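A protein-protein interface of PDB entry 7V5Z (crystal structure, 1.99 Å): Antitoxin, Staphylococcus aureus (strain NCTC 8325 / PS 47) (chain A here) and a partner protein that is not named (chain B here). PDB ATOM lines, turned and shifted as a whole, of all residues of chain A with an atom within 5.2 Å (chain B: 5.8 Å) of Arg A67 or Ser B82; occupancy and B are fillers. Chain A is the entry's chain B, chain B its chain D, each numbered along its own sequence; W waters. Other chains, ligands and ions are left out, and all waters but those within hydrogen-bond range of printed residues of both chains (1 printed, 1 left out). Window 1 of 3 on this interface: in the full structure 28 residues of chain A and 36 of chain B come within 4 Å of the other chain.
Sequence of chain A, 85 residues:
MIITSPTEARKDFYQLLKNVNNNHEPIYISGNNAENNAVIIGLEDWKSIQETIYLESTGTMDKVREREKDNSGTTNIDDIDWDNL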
ATOM      1  N   THR A  60     -27.933 -34.593  21.212  1.00  0.00           N
ATOM      2  CA  THR A  60     -27.820 -33.351  20.452  1.00  0.00           C
ATOM      3  C   THR A  60     -29.151 -32.966  19.823  1.00  0.00           C
ATOM      4  O   THR A  60     -29.555 -31.800  19.870  1.00  0.00           O
ATOM      5  CB  THR A  60     -26.741 -33.487  19.374  1.00  0.00           C
ATOM      6  OG1 THR A  60     -25.495 -33.837  19.980  1.00  0.00           O
ATOM      7  CG2 THR A  60     -26.569 -32.182  18.598  1.00  0.00           C
ATOM      8  N   ASP A  62     -32.123 -33.753  20.761  1.00  0.00           N
ATOM      9  CA  ASP A  62     -33.013 -33.296  21.829  1.00  0.00           C
ATOM     10  C   ASP A  62     -32.779 -31.825  22.123  1.00  0.00           C
ATOM     11  O   ASP A  62     -33.726 -31.039  22.255  1.00  0.00           O
ATOM     12  CB  ASP A  62     -32.785 -34.109  23.112  1.00  0.00           C
ATOM     13  CG  ASP A  62     -33.168 -35.564  22.974  1.00  0.00           C
ATOM     14  OD1 ASP A  62     -33.803 -35.929  21.964  1.00  0.00           O
ATOM     15  OD2 ASP A  62     -32.830 -36.347  23.892  1.00  0.00           O
ATOM     16  N   LYS A  63     -31.507 -31.450  22.269  1.00  0.00           N
ATOM     17  CA  LYS A  63     -31.141 -30.063  22.511  1.00  0.00           C
ATOM     18  C   LYS A  63     -31.584 -29.175  21.353  1.00  0.00           C
ATOM     19  O   LYS A  63     -32.124 -28.079  21.568  1.00  0.00           O
ATOM     20  CB  LYS A  63     -29.620 -29.993  22.742  1.00  0.00           C
ATOM     21  CG  LYS A  63     -29.061 -28.654  23.187  1.00  0.00           C
ATOM     22  CD  LYS A  63     -27.543 -28.777  23.502  1.00  0.00           C
ATOM     23  CE  LYS A  63     -26.690 -29.171  22.296  1.00  0.00           C
ATOM     24  NZ  LYS A  63     -25.210 -28.893  22.581  1.00  0.00           N
ATOM     25  N   VAL A  64     -31.420 -29.666  20.120  1.00  0.00           N
ATOM     26  CA  VAL A  64     -31.812 -28.908  18.924  1.00  0.00           C
ATOM     27  C   VAL A  64     -33.321 -28.663  18.904  1.00  0.00           C
ATOM     28  O   VAL A  64     -33.779 -27.533  18.686  1.00  0.00           O
ATOM     29  CB  VAL A  64     -31.342 -29.645  17.653  1.00  0.00           C
ATOM     30  CG1 VAL A  64     -32.068 -29.130  16.409  1.00  0.00           C
ATOM     31  CG2 VAL A  64     -29.821 -29.498  17.485  1.00  0.00           C
ATOM     32  N   ARG A  65     -34.116 -29.721  19.121  1.00  0.00           N
ATOM     33  CA  ARG A  65     -35.574 -29.571  19.091  1.00  0.00           C
ATOM     34  C   ARG A  65     -36.069 -28.637  20.186  1.00  0.00           C
ATOM     35  O   ARG A  65     -37.057 -27.922  19.990  1.00  0.00           O
ATOM     36  CB  ARG A  65     -36.272 -30.933  19.220  1.00  0.00           C
ATOM     37  CG  ARG A  65     -36.330 -31.774  17.916  1.00  0.00           C
ATOM     38  CD  ARG A  65     -37.004 -33.142  18.141  1.00  0.00           C
ATOM     39  NE  ARG A  65     -36.212 -34.027  19.005  1.00  0.00           N
ATOM     40  CZ  ARG A  65     -35.365 -34.951  18.556  1.00  0.00           C
ATOM     41  NH1 ARG A  65     -35.198 -35.124  17.248  1.00  0.00           N
ATOM     42  NH2 ARG A  65     -34.675 -35.701  19.410  1.00  0.00           N
ATOM     43  N   GLU A  66     -35.418 -28.636  21.345  1.00  0.00           N
ATOM     44  CA  GLU A  66     -35.836 -27.724  22.409  1.00  0.00           C
ATOM     45  C   GLU A  66     -35.461 -26.289  22.058  1.00  0.00           C
ATOM     46  O   GLU A  66     -36.243 -25.355  22.295  1.00  0.00           O
ATOM     47  CB  GLU A  66     -35.218 -28.166  23.747  1.00  0.00           C
ATOM     48  CG  GLU A  66     -35.568 -27.292  24.992  1.00  0.00           C
ATOM     49  CD  GLU A  66     -37.034 -27.413  25.417  1.00  0.00           C
ATOM     50  OE1 GLU A  66     -37.737 -28.333  24.944  1.00  0.00           O
ATOM     51  OE2 GLU A  66     -37.491 -26.581  26.216  1.00  0.00           O
ATOM     52  N   ARG A  67     -34.291 -26.098  21.447  1.00  0.00           N
ATOM     53  CA  ARG A  67     -33.871 -24.759  21.035  1.00  0.00           C
ATOM     54  C   ARG A  67     -34.750 -24.201  19.923  1.00  0.00           C
ATOM     55  O   ARG A  67     -35.033 -22.995  19.900  1.00  0.00           O
ATOM     56  CB  ARG A  67     -32.404 -24.786  20.601  1.00  0.00           C
ATOM     57  CG  ARG A  67     -31.465 -24.895  21.770  1.00  0.00           C
ATOM     58  CD  ARG A  67     -30.044 -25.134  21.342  1.00  0.00           C
ATOM     59  NE  ARG A  67     -29.143 -25.138  22.488  1.00  0.00           N
ATOM     60  CZ  ARG A  67     -27.843 -25.367  22.382  1.00  0.00           C
ATOM     61  NH1 ARG A  67     -27.326 -25.606  21.189  1.00  0.00           N
ATOM     62  NH2 ARG A  67     -27.058 -25.356  23.458  1.00  0.00           N
ATOM     63  N   GLU A  68     -35.187 -25.051  18.984  1.00  0.00           N
ATOM     64  CA  GLU A  68     -36.169 -24.597  18.001  1.00  0.00           C
ATOM     65  C   GLU A  68     -37.426 -24.081  18.678  1.00  0.00           C
ATOM     66  O   GLU A  68     -38.095 -23.185  18.146  1.00  0.00           O
ATOM     67  CB  GLU A  68     -36.542 -25.723  17.036  1.00  0.00           C
ATOM     68  CG  GLU A  68     -35.461 -26.121  16.065  1.00  0.00           C
ATOM     69  CD  GLU A  68     -35.838 -27.362  15.258  1.00  0.00           C
ATOM     70  OE1 GLU A  68     -36.699 -28.140  15.728  1.00  0.00           O
ATOM     71  OE2 GLU A  68     -35.267 -27.567  14.164  1.00  0.00           O
ATOM     72  N   LYS A  69     -37.765 -24.634  19.849  1.00  0.00           N
ATOM     73  CA  LYS A  69     -38.987 -24.242  20.547  1.00  0.00           C
ATOM     74  C   LYS A  69     -38.815 -22.967  21.373  1.00  0.00           C
ATOM     75  O   LYS A  69     -39.783 -22.233  21.564  1.00  0.00           O
ATOM     76  CB  LYS A  69     -39.463 -25.376  21.459  1.00  0.00           C
ATOM     77  CG  LYS A  69     -39.973 -26.624  20.756  1.00  0.00           C
ATOM     78  CD  LYS A  69     -40.212 -27.749  21.791  1.00  0.00           C
ATOM     79  CE  LYS A  69     -40.607 -29.040  21.083  1.00  0.00           C
ATOM     80  NZ  LYS A  69     -40.684 -30.187  22.038  1.00  0.00           N
ATOM     81  N   ASP A  70     -37.622 -22.683  21.882  1.00  0.00           N
ATOM     82  CA  ASP A  70     -37.497 -21.593  22.838  1.00  0.00           C
ATOM     83  C   ASP A  70     -37.596 -20.240  22.134  1.00  0.00           C
ATOM     84  O   ASP A  70     -37.578 -20.142  20.905  1.00  0.00           O
ATOM     85  CB  ASP A  70     -36.189 -21.711  23.631  1.00  0.00           C
ATOM     86  CG  ASP A  70     -34.942 -21.389  22.804  1.00  0.00           C
ATOM     87  OD1 ASP A  70     -34.907 -20.387  22.050  1.00  0.00           O
ATOM     88  OD2 ASP A  70     -33.953 -22.133  22.958  1.00  0.00           O
ATOM     89  N   LYS B   9     -29.112 -19.565  17.047  1.00  0.00           N
ATOM     90  CA  LYS B   9     -30.035 -19.423  18.160  1.00  0.00           C
ATOM     91  C   LYS B   9     -29.266 -18.968  19.398  1.00  0.00           C
ATOM     92  O   LYS B   9     -28.220 -19.532  19.734  1.00  0.00           O
ATOM     93  CB  LYS B   9     -30.753 -20.747  18.423  1.00  0.00           C
ATOM     94  CG  LYS B   9     -32.098 -20.574  19.084  1.00  0.00           C
ATOM     95  CD  LYS B   9     -33.182 -20.198  18.100  1.00  0.00           C
ATOM     96  CE  LYS B   9     -34.372 -19.622  18.851  1.00  0.00           C
ATOM     97  NZ  LYS B   9     -35.501 -20.572  18.965  1.00  0.00           N
ATOM     98  N   SER B  11     -29.773 -19.320  22.468  1.00  0.00           N
ATOM     99  CA  SER B  11     -29.557 -20.438  23.383  1.00  0.00           C
ATOM    100  C   SER B  11     -28.424 -21.355  22.940  1.00  0.00           C
ATOM    101  O   SER B  11     -27.958 -22.166  23.741  1.00  0.00           O
ATOM    102  CB  SER B  11     -30.840 -21.260  23.541  1.00  0.00           C
ATOM    103  OG  SER B  11     -31.371 -21.598  22.275  1.00  0.00           O
ATOM    104  N   ALA B  12     -27.968 -21.269  21.692  1.00  0.00           N
ATOM    105  CA  ALA B  12     -26.845 -22.102  21.275  1.00  0.00           C
ATOM    106  C   ALA B  12     -25.502 -21.431  21.516  1.00  0.00           C
ATOM    107  O   ALA B  12     -24.459 -22.030  21.236  1.00  0.00           O
ATOM    108  CB  ALA B  12     -26.972 -22.477  19.790  1.00  0.00           C
ATOM    109  N   LYS B  13     -25.491 -20.201  22.025  1.00  0.00           N
ATOM    110  CA  LYS B  13     -24.211 -19.529  22.246  1.00  0.00           C
ATOM    111  C   LYS B  13     -23.345 -20.267  23.269  1.00  0.00           C
ATOM    112  O   LYS B  13     -22.121 -20.287  23.126  1.00  0.00           O
ATOM    113  CB  LYS B  13     -24.450 -18.068  22.648  1.00  0.00           C
ATOM    114  CG  LYS B  13     -25.010 -17.243  21.482  1.00  0.00           C
ATOM    115  CD  LYS B  13     -24.821 -15.748  21.670  1.00  0.00           C
ATOM    116  CE  LYS B  13     -25.998 -15.131  22.400  1.00  0.00           C
ATOM    117  NZ  LYS B  13     -25.894 -13.632  22.486  1.00  0.00           N
ATOM    118  N   SER B  14     -23.950 -20.924  24.275  1.00  0.00           N
ATOM    119  CA  SER B  14     -23.131 -21.728  25.189  1.00  0.00           C
ATOM    120  C   SER B  14     -22.321 -22.784  24.439  1.00  0.00           C
ATOM    121  O   SER B  14     -21.208 -23.120  24.862  1.00  0.00           O
ATOM    122  CB  SER B  14     -23.993 -22.392  26.267  1.00  0.00           C
ATOM    123  OG  SER B  14     -25.081 -23.112  25.709  1.00  0.00           O
ATOM    124  N   ASP B  15     -22.855 -23.308  23.321  1.00  0.00           N
ATOM    125  CA  ASP B  15     -22.085 -24.211  22.469  1.00  0.00           C
ATOM    126  C   ASP B  15     -20.799 -23.557  21.988  1.00  0.00           C
ATOM    127  O   ASP B  15     -19.747 -24.208  21.937  1.00  0.00           O
ATOM    128  CB  ASP B  15     -22.904 -24.648  21.248  1.00  0.00           C
ATOM    129  CG  ASP B  15     -23.983 -25.664  21.572  1.00  0.00           C
ATOM    130  OD1 ASP B  15     -24.172 -26.013  22.758  1.00  0.00           O
ATOM    131  OD2 ASP B  15     -24.660 -26.115  20.620  1.00  0.00           O
ATOM    132  N   PHE B  28     -15.035 -24.277  13.193  1.00  0.00           N
ATOM    133  CA  PHE B  28     -16.431 -23.862  13.192  1.00  0.00           C
ATOM    134  C   PHE B  28     -16.673 -22.738  12.189  1.00  0.00           C
ATOM    135  O   PHE B  28     -17.630 -22.789  11.407  1.00  0.00           O
ATOM    136  CB  PHE B  28     -16.859 -23.421  14.586  1.00  0.00           C
ATOM    137  CG  PHE B  28     -18.194 -22.763  14.603  1.00  0.00           C
ATOM    138  CD1 PHE B  28     -19.349 -23.522  14.482  1.00  0.00           C
ATOM    139  CD2 PHE B  28     -18.301 -21.387  14.706  1.00  0.00           C
ATOM    140  CE1 PHE B  28     -20.587 -22.907  14.467  1.00  0.00           C
ATOM    141  CE2 PHE B  28     -19.527 -20.771  14.704  1.00  0.00           C
ATOM    142  CZ  PHE B  28     -20.670 -21.517  14.576  1.00  0.00           C
ATOM    143  N   ARG B  66     -20.672 -31.582  15.632  1.00  0.00           N
ATOM    144  CA  ARG B  66     -21.334 -31.131  14.424  1.00  0.00           C
ATOM    145  C   ARG B  66     -21.910 -29.743  14.641  1.00  0.00           C
ATOM    146  O   ARG B  66     -22.207 -29.337  15.773  1.00  0.00           O
ATOM    147  CB  ARG B  66     -22.480 -32.077  14.017  1.00  0.00           C
ATOM    148  CG  ARG B  66     -22.145 -33.545  14.163  1.00  0.00           C
ATOM    149  CD  ARG B  66     -21.166 -33.992  13.104  1.00  0.00           C
ATOM    150  NE  ARG B  66     -21.246 -35.438  12.955  1.00  0.00           N
ATOM    151  CZ  ARG B  66     -20.357 -36.282  13.460  1.00  0.00           C
ATOM    152  NH1 ARG B  66     -19.309 -35.812  14.126  1.00  0.00           N
ATOM    153  NH2 ARG B  66     -20.515 -37.587  13.298  1.00  0.00           N
ATOM    154  N   VAL B  67     -22.036 -29.021  13.539  1.00  0.00           N
ATOM    155  CA  VAL B  67     -22.959 -27.902  13.431  1.00  0.00           C
ATOM    156  C   VAL B  67     -24.255 -28.484  12.892  1.00  0.00           C
ATOM    157  O   VAL B  67     -24.259 -29.077  11.807  1.00  0.00           O
ATOM    158  CB  VAL B  67     -22.419 -26.815  12.490  1.00  0.00           C
ATOM    159  CG1 VAL B  67     -23.435 -25.691  12.344  1.00  0.00           C
ATOM    160  CG2 VAL B  67     -21.078 -26.283  12.988  1.00  0.00           C
ATOM    161  N   VAL B  68     -25.334 -28.380  13.662  1.00  0.00           N
ATOM    162  CA  VAL B  68     -26.657 -28.797  13.206  1.00  0.00           C
ATOM    163  C   VAL B  68     -27.462 -27.545  12.895  1.00  0.00           C
ATOM    164  O   VAL B  68     -27.441 -26.573  13.665  1.00  0.00           O
ATOM    165  CB  VAL B  68     -27.371 -29.682  14.249  1.00  0.00           C
ATOM    166  CG1 VAL B  68     -28.740 -30.092  13.742  1.00  0.00           C
ATOM    167  CG2 VAL B  68     -26.550 -30.953  14.549  1.00  0.00           C
ATOM    168  N   TYR B  69     -28.144 -27.542  11.747  1.00  0.00           N
ATOM    169  CA  TYR B  69     -28.762 -26.310  11.279  1.00  0.00           C
ATOM    170  C   TYR B  69     -29.984 -26.601  10.415  1.00  0.00           C
ATOM    171  O   TYR B  69     -30.147 -27.691   9.876  1.00  0.00           O
ATOM    172  CB  TYR B  69     -27.762 -25.454  10.485  1.00  0.00           C
ATOM    173  CG  TYR B  69     -27.191 -26.087   9.217  1.00  0.00           C
ATOM    174  CD1 TYR B  69     -26.098 -26.956   9.271  1.00  0.00           C
ATOM    175  CD2 TYR B  69     -27.733 -25.790   7.972  1.00  0.00           C
ATOM    176  CE1 TYR B  69     -25.562 -27.520   8.113  1.00  0.00           C
ATOM    177  CE2 TYR B  69     -27.206 -26.339   6.810  1.00  0.00           C
ATOM    178  CZ  TYR B  69     -26.127 -27.203   6.888  1.00  0.00           C
ATOM    179  OH  TYR B  69     -25.613 -27.739   5.739  1.00  0.00           O
ATOM    180  N   ILE B  80     -28.333 -21.899  12.760  1.00  0.00           N
ATOM    181  CA  ILE B  80     -27.517 -22.850  13.511  1.00  0.00           C
ATOM    182  C   ILE B  80     -28.195 -23.135  14.848  1.00  0.00           C
ATOM    183  O   ILE B  80     -28.506 -22.212  15.609  1.00  0.00           O
ATOM    184  CB  ILE B  80     -26.096 -22.302  13.720  1.00  0.00           C
ATOM    185  CG1 ILE B  80     -25.378 -22.159  12.376  1.00  0.00           C
ATOM    186  CG2 ILE B  80     -25.313 -23.192  14.708  1.00  0.00           C
ATOM    187  CD1 ILE B  80     -24.008 -21.557  12.494  1.00  0.00           C
ATOM    188  N   LEU B  81     -28.426 -24.418  15.136  1.00  0.00           N
ATOM    189  CA  LEU B  81     -29.098 -24.832  16.358  1.00  0.00           C
ATOM    190  C   LEU B  81     -28.180 -25.538  17.345  1.00  0.00           C
ATOM    191  O   LEU B  81     -28.488 -25.574  18.542  1.00  0.00           O
ATOM    192  CB  LEU B  81     -30.287 -25.734  16.007  1.00  0.00           C
ATOM    193  CG  LEU B  81     -31.346 -24.908  15.275  1.00  0.00           C
ATOM    194  CD1 LEU B  81     -32.195 -25.735  14.325  1.00  0.00           C
ATOM    195  CD2 LEU B  81     -32.223 -24.171  16.275  1.00  0.00           C
ATOM    196  N   SER B  82     -27.061 -26.084  16.887  1.00  0.00           N
ATOM    197  CA  SER B  82     -26.101 -26.692  17.793  1.00  0.00           C
ATOM    198  C   SER B  82     -24.748 -26.616  17.127  1.00  0.00           C
ATOM    199  O   SER B  82     -24.647 -26.759  15.903  1.00  0.00           O
ATOM    200  CB  SER B  82     -26.440 -28.152  18.123  1.00  0.00           C
ATOM    201  OG  SER B  82     -25.466 -28.726  18.994  1.00  0.00           O
ATOM    202  N   ALA B  83     -23.725 -26.350  17.935  1.00  0.00           N
ATOM    203  CA  ALA B  83     -22.347 -26.413  17.480  1.00  0.00           C
ATOM    204  C   ALA B  83     -21.518 -27.272  18.416  1.00  0.00           C
ATOM    205  O   ALA B  83     -20.290 -27.202  18.380  1.00  0.00           O
ATOM    206  CB  ALA B  83     -21.739 -25.012  17.362  1.00  0.00           C
ATOM    207  N   TRP B  84     -22.177 -28.079  19.246  1.00  0.00           N
ATOM    208  CA  TRP B  84     -21.522 -28.942  20.228  1.00  0.00           C
ATOM    209  C   TRP B  84     -22.392 -30.182  20.393  1.00  0.00           C
ATOM    210  O   TRP B  84     -23.564 -30.062  20.761  1.00  0.00           O
ATOM    211  CB  TRP B  84     -21.365 -28.208  21.567  1.00  0.00           C
ATOM    212  CG  TRP B  84     -20.524 -28.925  22.603  1.00  0.00           C
ATOM    213  CD1 TRP B  84     -20.976 -29.614  23.701  1.00  0.00           C
ATOM    214  CD2 TRP B  84     -19.095 -28.991  22.652  1.00  0.00           C
ATOM    215  NE1 TRP B  84     -19.916 -30.112  24.415  1.00  0.00           N
ATOM    216  CE2 TRP B  84     -18.749 -29.740  23.800  1.00  0.00           C
ATOM    217  CE3 TRP B  84     -18.070 -28.489  21.838  1.00  0.00           C
ATOM    218  CZ2 TRP B  84     -17.433 -30.002  24.147  1.00  0.00           C
ATOM    219  CZ3 TRP B  84     -16.756 -28.754  22.185  1.00  0.00           C
ATOM    220  CH2 TRP B  84     -16.451 -29.499  23.330  1.00  0.00           C
ATOM    221  N   SER B  85     -21.836 -31.365  20.135  1.00  0.00           N
ATOM    222  CA  SER B  85     -22.656 -32.582  20.077  1.00  0.00           C
ATOM    223  C   SER B  85     -22.737 -33.242  21.455  1.00  0.00           C
ATOM    224  O   SER B  85     -22.031 -34.198  21.778  1.00  0.00           O
ATOM    225  CB  SER B  85     -22.124 -33.532  19.011  1.00  0.00           C
ATOM    226  OG  SER B  85     -22.126 -32.857  17.755  1.00  0.00           O
ATOM    227  N   HIS B  86     -23.689 -32.754  22.241  1.00  0.00           N
ATOM    228  CA  HIS B  86     -23.877 -33.155  23.627  1.00  0.00           C
ATOM    229  C   HIS B  86     -25.292 -32.767  24.025  1.00  0.00           C
ATOM    230  O   HIS B  86     -25.927 -31.939  23.364  1.00  0.00           O
ATOM    231  CB  HIS B  86     -22.838 -32.486  24.530  1.00  0.00           C
ATOM    232  CG  HIS B  86     -22.814 -33.007  25.930  1.00  0.00           C
ATOM    233  ND1 HIS B  86     -22.834 -32.178  27.034  1.00  0.00           N
ATOM    234  CD2 HIS B  86     -22.757 -34.270  26.408  1.00  0.00           C
ATOM    235  CE1 HIS B  86     -22.802 -32.910  28.134  1.00  0.00           C
ATOM    236  NE2 HIS B  86     -22.752 -34.182  27.782  1.00  0.00           N
ATOM    237  N   ASP B  88     -26.283 -31.072  26.612  1.00  0.00           N
ATOM    238  CA  ASP B  88     -26.420 -29.643  26.915  1.00  0.00           C
ATOM    239  C   ASP B  88     -25.265 -28.807  26.328  1.00  0.00           C
ATOM    240  O   ASP B  88     -24.460 -29.297  25.519  1.00  0.00           O
ATOM    241  CB  ASP B  88     -26.574 -29.401  28.432  1.00  0.00           C
ATOM    242  CG  ASP B  88     -25.398 -29.906  29.246  1.00  0.00           C
ATOM    243  OD1 ASP B  88     -24.262 -29.918  28.728  1.00  0.00           O
ATOM    244  OD2 ASP B  88     -25.619 -30.293  30.416  1.00  0.00           O
ATOM    245  OXT ASP B  88     -25.131 -27.609  26.617  1.00  0.00           O
HETATM  246  O   HOH W   1     -36.294 -21.402  16.267  1.00  0.00           O
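Of the 10 printed residues of chain A, 6 touch a printed residue of chain B. Printed residues of chain B that touch a printed residue of chain A: Lys B9, Ser B11, Ala B12, Ser B14, Asp B15, Val B68, Leu B81, Ser B82, Trp B84, Ser B85, His B86 and Asp B88. Hydrophobic or aromatic side chains of chain B within 4 Å of the printed part of chain A: Ala B12, Val B68 and Leu B81. Among the printed residues, 22 pairs touch across the chains. Among the printed residues, Asp or Glu carboxylates within 4 Å of a Lys or Arg side-chain nitrogen of the other chain: Lys A63 with Asp B15 (3.1 Å), Arg A67 with Asp B15 (2.8 Å) and Asp A70 with Lys B9 (3.1 Å).
OD2 of Asp B15 lies within hydrogen-bond range of OG of Ser B82 (3.2 Å). N of Ala B83 is in hydrogen-bond range of OD2 of Asp B15, 2.9 Å away. The backbone NH (N) of Arg B66 lies within hydrogen-bond range of the side-chain hydroxyl (OG) of Ser B85 (2.9 Å). O of Val B68 lies within hydrogen-bond range of N of Leu B81 (2.8 Å). The side-chain hydroxyl of Ser B82 sits at hydrogen-bond distance from the backbone carbonyl oxygen of Trp B84, at 2.9 Å. The side-chain carboxylate (OD1) of Asp B88 lies within hydrogen-bond range of a ring nitrogen (ND1) of His B86, at 3.2 Å.
Arg A67 touches seven residues of chain B. Ser B82 touches four residues of chain A. Of the printed residues of chain B, Glu A68 touches Lys B9 (3.8 Å) and Leu B81 (3.6 Å). Printed residues of chain A within 4 Å of Ser B14: Arg A67. Phe B28 touches none of the printed residues of chain A. Asp A62 touches none of the printed residues of chain B. The nearest residue of chain B that does not touch Arg A67 is Asp B88 (4.3 Å). The nearest printed residue of chain B that does not touch Thr A60 is Val B68 (4.2 Å).
OG1 of Thr A60 is in hydrogen-bond range of N of His B86 (3.1 Å). The side-chain amino group (NZ) of Lys A63 lies within salt-bridge range of the side-chain carboxylate (OD1) of Asp B15 (3.1 Å). The backbone carbonyl oxygen of Trp B84 is in hydrogen-bond range of the side-chain amino group of Lys A63, at 2.7 Å. The side-chain amino group of Lys A63 sits close to the backbone carbonyl oxygen of His B86 (3.2 Å). The side-chain amino group (NZ) of Lys A63 is in salt-bridge range of the chain-end carboxylate (O) of Asp B88, 3.1 Å away. The backbone carbonyl oxygen (O) of Arg A67 is in hydrogen-bond range of the side-chain amino group (NZ) of Lys B9 (2.6 Å). NH2 of Arg A67 is in hydrogen-bond range of O of Ser B11 (3.3 Å). The guanidinium group of Arg A67 is in salt-bridge range of the side-chain carboxylate of Asp B15, 2.8 Å away. The guanidinium group (NH1) of Arg A67 is in hydrogen-bond range of the backbone carbonyl oxygen (O) of Leu B81 (2.9 Å). NZ of Lys B9 is in salt-bridge range of OD1 of Asp A70 (3.1 Å). OG of Ser B11 lies within hydrogen-bond range of OD2 of Asp A70 (2.7 Å).
Water W1 bridges NZ of Lys B9 (2.9 Å) and O of Glu A68 (3.2 Å).
OG of Ser B82 touches CG2 of Thr A60, 3.6 Å away. Ser B85 touches Thr A60 (CA to OG1, 3.1 Å). CG1 of Val B68 touches CG2 of Val A64 (3.9 Å). Val A64 touches Leu B81 (CG1 to CB, 3.9 Å). Val A64 touches Ser B82. NH1 of Arg A67 touches CB of Ala B12 (3.4 Å). Ser B14 touches Arg A67. Ser B82 touches Arg A67 (CA to NH1, 3.8 Å). O of Glu A68 touches NZ of Lys B9, at 3.8 Å. Glu A68 touches Leu B81 (OE2 to CD1, 3.6 Å).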
